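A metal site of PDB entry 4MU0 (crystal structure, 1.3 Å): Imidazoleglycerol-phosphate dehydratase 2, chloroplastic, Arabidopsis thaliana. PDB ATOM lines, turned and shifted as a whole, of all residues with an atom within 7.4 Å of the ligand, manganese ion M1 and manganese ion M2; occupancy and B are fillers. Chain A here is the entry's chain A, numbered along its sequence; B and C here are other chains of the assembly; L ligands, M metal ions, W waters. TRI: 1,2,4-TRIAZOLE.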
ATOM      1  N   GLU A  19     -23.217  20.218  30.077  1.00  0.00           N
ATOM      2  CA  GLU A  19     -22.077  19.338  29.755  1.00  0.00           C
ATOM      3  C   GLU A  19     -20.953  19.292  30.814  1.00  0.00           C
ATOM      4  O   GLU A  19     -20.299  18.283  30.958  1.00  0.00           O
ATOM      5  CB  GLU A  19     -21.470  19.759  28.385  1.00  0.00           C
ATOM      6  CG  GLU A  19     -22.416  19.592  27.175  1.00  0.00           C
ATOM      7  CD  GLU A  19     -23.360  20.754  26.975  1.00  0.00           C
ATOM      8  OE1 GLU A  19     -23.069  21.853  27.504  1.00  0.00           O
ATOM      9  OE2 GLU A  19     -24.387  20.575  26.280  1.00  0.00           O
ATOM     10  N   ASP A  65     -18.488  15.680  30.694  1.00  0.00           N
ATOM     11  CA  ASP A  65     -18.946  14.544  29.875  1.00  0.00           C
ATOM     12  C   ASP A  65     -17.838  13.849  29.097  1.00  0.00           C
ATOM     13  O   ASP A  65     -17.913  13.648  27.891  1.00  0.00           O
ATOM     14  CB  ASP A  65     -20.126  14.949  28.997  1.00  0.00           C
ATOM     15  CG  ASP A  65     -19.811  16.119  28.043  1.00  0.00           C
ATOM     16  OD1 ASP A  65     -18.669  16.591  27.982  1.00  0.00           O
ATOM     17  OD2 ASP A  65     -20.747  16.545  27.330  1.00  0.00           O
ATOM     18  N   ILE A  68     -18.154  11.101  26.415  1.00  0.00           N
ATOM     19  CA  ILE A  68     -18.361  11.491  25.026  1.00  0.00           C
ATOM     20  C   ILE A  68     -17.028  11.786  24.360  1.00  0.00           C
ATOM     21  O   ILE A  68     -16.745  11.254  23.314  1.00  0.00           O
ATOM     22  CB  ILE A  68     -19.282  12.721  24.933  1.00  0.00           C
ATOM     23  CG1 ILE A  68     -20.660  12.407  25.446  1.00  0.00           C
ATOM     24  CG2 ILE A  68     -19.352  13.246  23.504  1.00  0.00           C
ATOM     25  CD1 ILE A  68     -21.533  13.620  25.562  1.00  0.00           C
ATOM     26  N   ASP A  69     -16.278  12.686  24.970  1.00  0.00           N
ATOM     27  CA  ASP A  69     -14.866  12.903  24.708  1.00  0.00           C
ATOM     28  C   ASP A  69     -14.418  14.040  25.592  1.00  0.00           C
ATOM     29  O   ASP A  69     -15.213  14.561  26.369  1.00  0.00           O
ATOM     30  CB  ASP A  69     -14.482  13.094  23.247  1.00  0.00           C
ATOM     31  CG  ASP A  69     -14.921  14.413  22.670  1.00  0.00           C
ATOM     32  OD1 ASP A  69     -15.567  15.129  23.402  1.00  0.00           O
ATOM     33  OD2 ASP A  69     -14.628  14.769  21.458  1.00  0.00           O
ATOM     34  N   HIS A  71     -13.551  16.943  24.768  1.00  0.00           N
ATOM     35  CA  HIS A  71     -13.713  18.229  24.105  1.00  0.00           C
ATOM     36  C   HIS A  71     -14.467  19.264  24.934  1.00  0.00           C
ATOM     37  O   HIS A  71     -14.000  20.403  25.089  1.00  0.00           O
ATOM     38  CB  HIS A  71     -14.443  18.002  22.785  1.00  0.00           C
ATOM     39  CG  HIS A  71     -14.538  19.204  21.908  1.00  0.00           C
ATOM     40  ND1 HIS A  71     -14.090  19.187  20.619  1.00  0.00           N
ATOM     41  CD2 HIS A  71     -15.056  20.446  22.098  1.00  0.00           C
ATOM     42  CE1 HIS A  71     -14.321  20.357  20.055  1.00  0.00           C
ATOM     43  NE2 HIS A  71     -14.933  21.138  20.919  1.00  0.00           N
ATOM     44  N   HIS A  72     -15.674  18.921  25.413  1.00  0.00           N
ATOM     45  CA  HIS A  72     -16.446  19.968  26.090  1.00  0.00           C
ATOM     46  C   HIS A  72     -15.730  20.451  27.370  1.00  0.00           C
ATOM     47  O   HIS A  72     -15.723  21.629  27.678  1.00  0.00           O
ATOM     48  CB  HIS A  72     -17.870  19.488  26.425  1.00  0.00           C
ATOM     49  CG  HIS A  72     -18.695  19.059  25.249  1.00  0.00           C
ATOM     50  ND1 HIS A  72     -19.690  18.141  25.373  1.00  0.00           N
ATOM     51  CD2 HIS A  72     -18.677  19.388  23.938  1.00  0.00           C
ATOM     52  CE1 HIS A  72     -20.272  17.925  24.209  1.00  0.00           C
ATOM     53  NE2 HIS A  72     -19.677  18.676  23.314  1.00  0.00           N
ATOM     54  N   GLU A  75     -12.721  22.668  26.455  1.00  0.00           N
ATOM     55  CA  GLU A  75     -13.207  23.957  26.009  1.00  0.00           C
ATOM     56  C   GLU A  75     -13.695  24.828  27.156  1.00  0.00           C
ATOM     57  O   GLU A  75     -13.358  26.013  27.254  1.00  0.00           O
ATOM     58  CB  GLU A  75     -14.339  23.739  24.990  1.00  0.00           C
ATOM     59  CG  GLU A  75     -14.996  25.029  24.521  1.00  0.00           C
ATOM     60  CD  GLU A  75     -15.841  24.889  23.258  1.00  0.00           C
ATOM     61  OE1 GLU A  75     -15.893  23.769  22.714  1.00  0.00           O
ATOM     62  OE2 GLU A  75     -16.373  25.930  22.785  1.00  0.00           O
ATOM     63  N   LEU A 140      -7.120  19.061  20.704  1.00  0.00           N
ATOM     64  CA  LEU A 140      -7.665  19.893  21.754  1.00  0.00           C
ATOM     65  C   LEU A 140      -6.723  20.990  22.210  1.00  0.00           C
ATOM     66  O   LEU A 140      -7.146  21.934  22.872  1.00  0.00           O
ATOM     67  CB  LEU A 140      -8.165  19.035  22.898  1.00  0.00           C
ATOM     68  CG  LEU A 140      -9.267  18.057  22.482  1.00  0.00           C
ATOM     69  CD1 LEU A 140      -9.741  17.245  23.690  1.00  0.00           C
ATOM     70  CD2 LEU A 140     -10.475  18.771  21.891  1.00  0.00           C
ATOM     71  N   HIS A 143      -7.745  24.129  20.407  1.00  0.00           N
ATOM     72  CA  HIS A 143      -9.030  24.586  20.937  1.00  0.00           C
ATOM     73  C   HIS A 143      -8.905  25.226  22.329  1.00  0.00           C
ATOM     74  O   HIS A 143      -9.587  26.195  22.630  1.00  0.00           O
ATOM     75  CB  HIS A 143     -10.046  23.431  20.979  1.00  0.00           C
ATOM     76  CG  HIS A 143     -11.473  23.864  20.911  1.00  0.00           C
ATOM     77  ND1 HIS A 143     -11.968  24.987  21.546  1.00  0.00           N
ATOM     78  CD2 HIS A 143     -12.554  23.272  20.349  1.00  0.00           C
ATOM     79  CE1 HIS A 143     -13.272  25.069  21.317  1.00  0.00           C
ATOM     80  NE2 HIS A 143     -13.643  24.035  20.598  1.00  0.00           N
ATOM     81  N   SER A 147     -10.128  29.093  22.768  1.00  0.00           N
ATOM     82  CA  SER A 147     -11.155  29.411  23.714  1.00  0.00           C
ATOM     83  C   SER A 147     -10.654  30.397  24.788  1.00  0.00           C
ATOM     84  O   SER A 147     -11.334  31.344  25.139  1.00  0.00           O
ATOM     85  CB  SER A 147     -11.679  28.123  24.339  1.00  0.00           C
ATOM     86  OG  SER A 147     -12.379  27.339  23.393  1.00  0.00           O
ATOM     87  N   PHE B  42     -20.757   8.996  21.836  1.00  0.00           N
ATOM     88  CA  PHE B  42     -20.673  10.068  20.863  1.00  0.00           C
ATOM     89  C   PHE B  42     -21.923  10.067  19.942  1.00  0.00           C
ATOM     90  O   PHE B  42     -22.408  11.124  19.552  1.00  0.00           O
ATOM     91  CB  PHE B  42     -19.397  10.040  20.020  1.00  0.00           C
ATOM     92  CG  PHE B  42     -19.152  11.328  19.270  1.00  0.00           C
ATOM     93  CD1 PHE B  42     -18.567  12.386  19.889  1.00  0.00           C
ATOM     94  CD2 PHE B  42     -19.571  11.470  17.960  1.00  0.00           C
ATOM     95  CE1 PHE B  42     -18.383  13.590  19.253  1.00  0.00           C
ATOM     96  CE2 PHE B  42     -19.381  12.698  17.324  1.00  0.00           C
ATOM     97  CZ  PHE B  42     -18.813  13.752  17.981  1.00  0.00           C
ATOM     98  N   HIS B  45     -24.702  11.697  21.656  1.00  0.00           N
ATOM     99  CA  HIS B  45     -24.563  13.161  21.591  1.00  0.00           C
ATOM    100  C   HIS B  45     -25.062  13.682  20.229  1.00  0.00           C
ATOM    101  O   HIS B  45     -25.732  14.710  20.155  1.00  0.00           O
ATOM    102  CB  HIS B  45     -23.084  13.497  21.876  1.00  0.00           C
ATOM    103  CG  HIS B  45     -22.758  14.957  21.828  1.00  0.00           C
ATOM    104  ND1 HIS B  45     -23.553  15.923  22.404  1.00  0.00           N
ATOM    105  CD2 HIS B  45     -21.668  15.619  21.350  1.00  0.00           C
ATOM    106  CE1 HIS B  45     -22.983  17.119  22.233  1.00  0.00           C
ATOM    107  NE2 HIS B  45     -21.845  16.957  21.590  1.00  0.00           N
ATOM    108  N   MET B  46     -24.735  12.996  19.161  1.00  0.00           N
ATOM    109  CA  MET B  46     -25.206  13.408  17.836  1.00  0.00           C
ATOM    110  C   MET B  46     -26.715  13.266  17.686  1.00  0.00           C
ATOM    111  O   MET B  46     -27.362  14.123  17.091  1.00  0.00           O
ATOM    112  CB  MET B  46     -24.477  12.633  16.733  1.00  0.00           C
ATOM    113  CG  MET B  46     -22.995  12.921  16.620  1.00  0.00           C
ATOM    114  SD  MET B  46     -22.586  14.683  16.451  1.00  0.00           S
ATOM    115  CE  MET B  46     -22.244  15.148  18.172  1.00  0.00           C
ATOM    116  N   GLN B  49     -28.405  16.126  19.129  1.00  0.00           N
ATOM    117  CA  GLN B  49     -28.385  17.271  18.206  1.00  0.00           C
ATOM    118  C   GLN B  49     -29.492  17.161  17.183  1.00  0.00           C
ATOM    119  O   GLN B  49     -30.143  18.136  16.797  1.00  0.00           O
ATOM    120  CB  GLN B  49     -27.029  17.422  17.491  1.00  0.00           C
ATOM    121  CG  GLN B  49     -25.831  17.571  18.405  1.00  0.00           C
ATOM    122  CD  GLN B  49     -26.017  18.609  19.442  1.00  0.00           C
ATOM    123  OE1 GLN B  49     -26.383  19.732  19.126  1.00  0.00           O
ATOM    124  NE2 GLN B  49     -25.757  18.271  20.701  1.00  0.00           N
ATOM    125  N   LEU B 105     -20.127  25.116  12.915  1.00  0.00           N
ATOM    126  CA  LEU B 105     -19.800  24.940  14.313  1.00  0.00           C
ATOM    127  C   LEU B 105     -18.348  25.435  14.375  1.00  0.00           C
ATOM    128  O   LEU B 105     -17.420  24.778  13.920  1.00  0.00           O
ATOM    129  CB  LEU B 105     -19.921  23.517  14.828  1.00  0.00           C
ATOM    130  CG  LEU B 105     -19.912  23.446  16.359  1.00  0.00           C
ATOM    131  CD1 LEU B 105     -20.086  22.012  16.802  1.00  0.00           C
ATOM    132  CD2 LEU B 105     -18.816  24.128  17.102  1.00  0.00           C
ATOM    133  N   ASP B 106     -18.194  26.666  14.844  1.00  0.00           N
ATOM    134  CA  ASP B 106     -16.915  27.355  14.846  1.00  0.00           C
ATOM    135  C   ASP B 106     -16.334  27.313  13.416  1.00  0.00           C
ATOM    136  O   ASP B 106     -16.974  27.813  12.484  1.00  0.00           O
ATOM    137  CB  ASP B 106     -15.974  26.862  15.949  1.00  0.00           C
ATOM    138  CG  ASP B 106     -16.499  27.097  17.341  1.00  0.00           C
ATOM    139  OD1 ASP B 106     -17.524  27.788  17.494  1.00  0.00           O
ATOM    140  OD2 ASP B 106     -15.838  26.604  18.273  1.00  0.00           O
ATOM    141  N   GLU B 107     -15.133  26.756  13.238  1.00  0.00           N
ATOM    142  CA  GLU B 107     -14.450  26.756  11.948  1.00  0.00           C
ATOM    143  C   GLU B 107     -15.061  25.775  10.957  1.00  0.00           C
ATOM    144  O   GLU B 107     -14.753  25.832   9.780  1.00  0.00           O
ATOM    145  CB  GLU B 107     -12.966  26.474  12.180  1.00  0.00           C
ATOM    146  CG  GLU B 107     -12.508  25.008  12.141  1.00  0.00           C
ATOM    147  CD  GLU B 107     -13.125  24.092  13.179  1.00  0.00           C
ATOM    148  OE1 GLU B 107     -13.571  24.589  14.225  1.00  0.00           O
ATOM    149  OE2 GLU B 107     -13.129  22.849  12.916  1.00  0.00           O
ATOM    150  N   ASN B 165     -11.485  20.518  13.305  1.00  0.00           N
ATOM    151  CA  ASN B 165     -11.729  19.726  14.499  1.00  0.00           C
ATOM    152  C   ASN B 165     -12.773  18.665  14.188  1.00  0.00           C
ATOM    153  O   ASN B 165     -13.848  18.973  13.694  1.00  0.00           O
ATOM    154  CB  ASN B 165     -12.173  20.637  15.633  1.00  0.00           C
ATOM    155  CG  ASN B 165     -12.455  19.843  16.903  1.00  0.00           C
ATOM    156  OD1 ASN B 165     -13.480  19.160  17.006  1.00  0.00           O
ATOM    157  ND2 ASN B 165     -11.509  19.861  17.812  1.00  0.00           N
ATOM    158  N   HIS B 167     -14.722  16.682  16.007  1.00  0.00           N
ATOM    159  CA  HIS B 167     -15.985  16.806  16.710  1.00  0.00           C
ATOM    160  C   HIS B 167     -16.816  17.932  16.092  1.00  0.00           C
ATOM    161  O   HIS B 167     -18.007  17.759  15.863  1.00  0.00           O
ATOM    162  CB  HIS B 167     -15.663  17.021  18.194  1.00  0.00           C
ATOM    163  CG  HIS B 167     -16.818  17.092  19.162  1.00  0.00           C
ATOM    164  ND1 HIS B 167     -16.685  16.562  20.442  1.00  0.00           N
ATOM    165  CD2 HIS B 167     -18.013  17.715  19.138  1.00  0.00           C
ATOM    166  CE1 HIS B 167     -17.793  16.843  21.132  1.00  0.00           C
ATOM    167  NE2 HIS B 167     -18.599  17.557  20.370  1.00  0.00           N
ATOM    168  N   HIS B 168     -16.195  19.051  15.783  1.00  0.00           N
ATOM    169  CA  HIS B 168     -16.903  20.135  15.117  1.00  0.00           C
ATOM    170  C   HIS B 168     -17.484  19.717  13.768  1.00  0.00           C
ATOM    171  O   HIS B 168     -18.617  20.041  13.429  1.00  0.00           O
ATOM    172  CB  HIS B 168     -16.047  21.370  14.927  1.00  0.00           C
ATOM    173  CG  HIS B 168     -15.687  22.067  16.208  1.00  0.00           C
ATOM    174  ND1 HIS B 168     -14.853  23.148  16.246  1.00  0.00           N
ATOM    175  CD2 HIS B 168     -16.087  21.854  17.481  1.00  0.00           C
ATOM    176  CE1 HIS B 168     -14.752  23.598  17.495  1.00  0.00           C
ATOM    177  NE2 HIS B 168     -15.484  22.821  18.266  1.00  0.00           N
ATOM    178  N   GLU B 171     -20.420  17.199  14.348  1.00  0.00           N
ATOM    179  CA  GLU B 171     -21.557  17.840  15.001  1.00  0.00           C
ATOM    180  C   GLU B 171     -22.242  18.835  14.078  1.00  0.00           C
ATOM    181  O   GLU B 171     -23.486  18.853  14.008  1.00  0.00           O
ATOM    182  CB  GLU B 171     -21.177  18.443  16.332  1.00  0.00           C
ATOM    183  CG  GLU B 171     -22.377  18.929  17.115  1.00  0.00           C
ATOM    184  CD  GLU B 171     -22.095  19.322  18.529  1.00  0.00           C
ATOM    185  OE1 GLU B 171     -21.184  18.737  19.110  1.00  0.00           O
ATOM    186  OE2 GLU B 171     -22.738  20.287  19.028  1.00  0.00           O
ATOM    187  N   LYS B 175     -26.168  18.973  12.868  1.00  0.00           N
ATOM    188  CA  LYS B 175     -26.969  20.174  12.961  1.00  0.00           C
ATOM    189  C   LYS B 175     -27.610  20.502  11.602  1.00  0.00           C
ATOM    190  O   LYS B 175     -28.799  20.797  11.505  1.00  0.00           O
ATOM    191  CB  LYS B 175     -26.174  21.390  13.429  1.00  0.00           C
ATOM    192  CG  LYS B 175     -25.725  21.254  14.881  1.00  0.00           C
ATOM    193  CD  LYS B 175     -24.900  22.441  15.373  1.00  0.00           C
ATOM    194  CE  LYS B 175     -24.415  22.258  16.844  1.00  0.00           C
ATOM    195  NZ  LYS B 175     -23.885  23.499  17.446  1.00  0.00           N
ATOM    196  N   ARG C 119     -19.669  32.277  20.485  1.00  0.00           N
ATOM    197  CA  ARG C 119     -18.250  31.990  20.274  1.00  0.00           C
ATOM    198  C   ARG C 119     -17.817  32.729  18.998  1.00  0.00           C
ATOM    199  O   ARG C 119     -18.338  32.434  17.929  1.00  0.00           O
ATOM    200  CB  ARG C 119     -18.044  30.501  20.065  1.00  0.00           C
ATOM    201  CG  ARG C 119     -18.415  29.664  21.259  1.00  0.00           C
ATOM    202  CD  ARG C 119     -18.128  28.190  21.019  1.00  0.00           C
ATOM    203  NE  ARG C 119     -18.925  27.680  19.938  1.00  0.00           N
ATOM    204  CZ  ARG C 119     -20.099  27.109  20.084  1.00  0.00           C
ATOM    205  NH1 ARG C 119     -20.618  26.872  21.287  1.00  0.00           N
ATOM    206  NH2 ARG C 119     -20.789  26.741  19.022  1.00  0.00           N
HETATM  207  N1  TRI L   1     -19.370  20.666  20.764  1.00  0.00           N
HETATM  208  N2  TRI L   1     -19.978  21.896  20.798  1.00  0.00           N
HETATM  209  C3  TRI L   1     -18.955  22.790  20.675  1.00  0.00           C
HETATM  210  N4  TRI L   1     -17.805  22.176  20.603  1.00  0.00           N
HETATM  211  C5  TRI L   1     -18.058  20.859  20.624  1.00  0.00           C
HETATM  212 MN    MN M   1     -15.791  23.175  20.498  1.00  0.00          MN
HETATM  213 MN    MN M   2     -20.438  18.713  21.154  1.00  0.00          MN
HETATM  214  O   HOH W   1     -16.804  25.086  20.263  1.00  0.00           O
HETATM  215  O   HOH W   2     -22.200  20.058  21.700  1.00  0.00           O
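Four residues have an atom within 4 Å of manganese ion M2: His 72, His 45 of chain B, His 167 of chain B and Glu 171 of chain B.
CD2 of Leu 105 of chain B touches C3 of the ligand, at 3.8 Å. Seven residues have an atom within 4 Å of the ligand: His 71, His 72, Glu 75, Leu 105 of chain B, His 167 of chain B, His 168 of chain B and Glu 171 of chain B. The nearest printed residue that does not touch the ligand is Arg 119 of chain C (4.5 Å).
Of the 23 residues printed, 4 come within 4 Å of manganese ion M1. The nearest printed residue that does not touch manganese ion M1 is Asp 106 of chain B (4.1 Å).
The backbone NH of His 168 of chain B sits at hydrogen-bond distance from the side-chain amide oxygen of Asn 165 of chain B (3.0 Å). ND1 of His 168 of chain B is in hydrogen-bond range of OE1 of Glu 107 of chain B, at 2.8 Å. The side-chain hydroxyl of Ser 147 lies within hydrogen-bond range of a ring nitrogen (ND1) of His 143, 3.0 Å away. The backbone NH (N) of His 71 lies within hydrogen-bond range of the side-chain carboxylate (OD1) of Asp 69, 3.0 Å away. ND1 of His 72 is in hydrogen-bond range of OD2 of Asp 65. The backbone NH (N) of His 167 of chain B sits at hydrogen-bond distance from the side-chain amide oxygen (OD1) of Asn 165 of chain B, 2.9 Å away. ND1 of His 167 of chain B sits at hydrogen-bond distance from OD2 of Asp 69.
Water W1 lies within hydrogen-bond range of the side-chain carboxylate (OD2) of Asp 106 of chain B (2.7 Å), the side-chain carboxylate (OE2) of Glu 75 (2.7 Å) and the guanidinium group (NE) of Arg 119 of chain C (3.4 Å). Water W2 lies within hydrogen-bond range of the side-chain carboxylate (OE2) of Glu 171 of chain B (2.7 Å) and a nitrogen (N2) of the ligand (3.0 Å).
Manganese ion M2 is bound by the side-chain carboxylate of Glu 171 of chain B (2.2 Å), a nitrogen (N1) of the ligand (2.3 Å), water W2 (2.3 Å), a ring nitrogen (NE2) of His 72 (2.3 Å), a ring nitrogen (NE2) of His 45 of chain B (2.3 Å) and a ring nitrogen (NE2) of His 167 of chain B (2.3 Å). Manganese ion M2 has six donor atoms within binding distance.
Manganese ion M1 is bound by water W1 (2.2 Å), a ring nitrogen (NE2) of His 71 (2.3 Å), a nitrogen (N4) of the ligand (2.3 Å), a ring nitrogen (NE2) of His 168 of chain B (2.3 Å), the side-chain carboxylate of Glu 75 (2.3 Å) and a ring nitrogen (NE2) of His 143 (2.3 Å). Manganese ion M1 has six donor atoms within binding distance.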
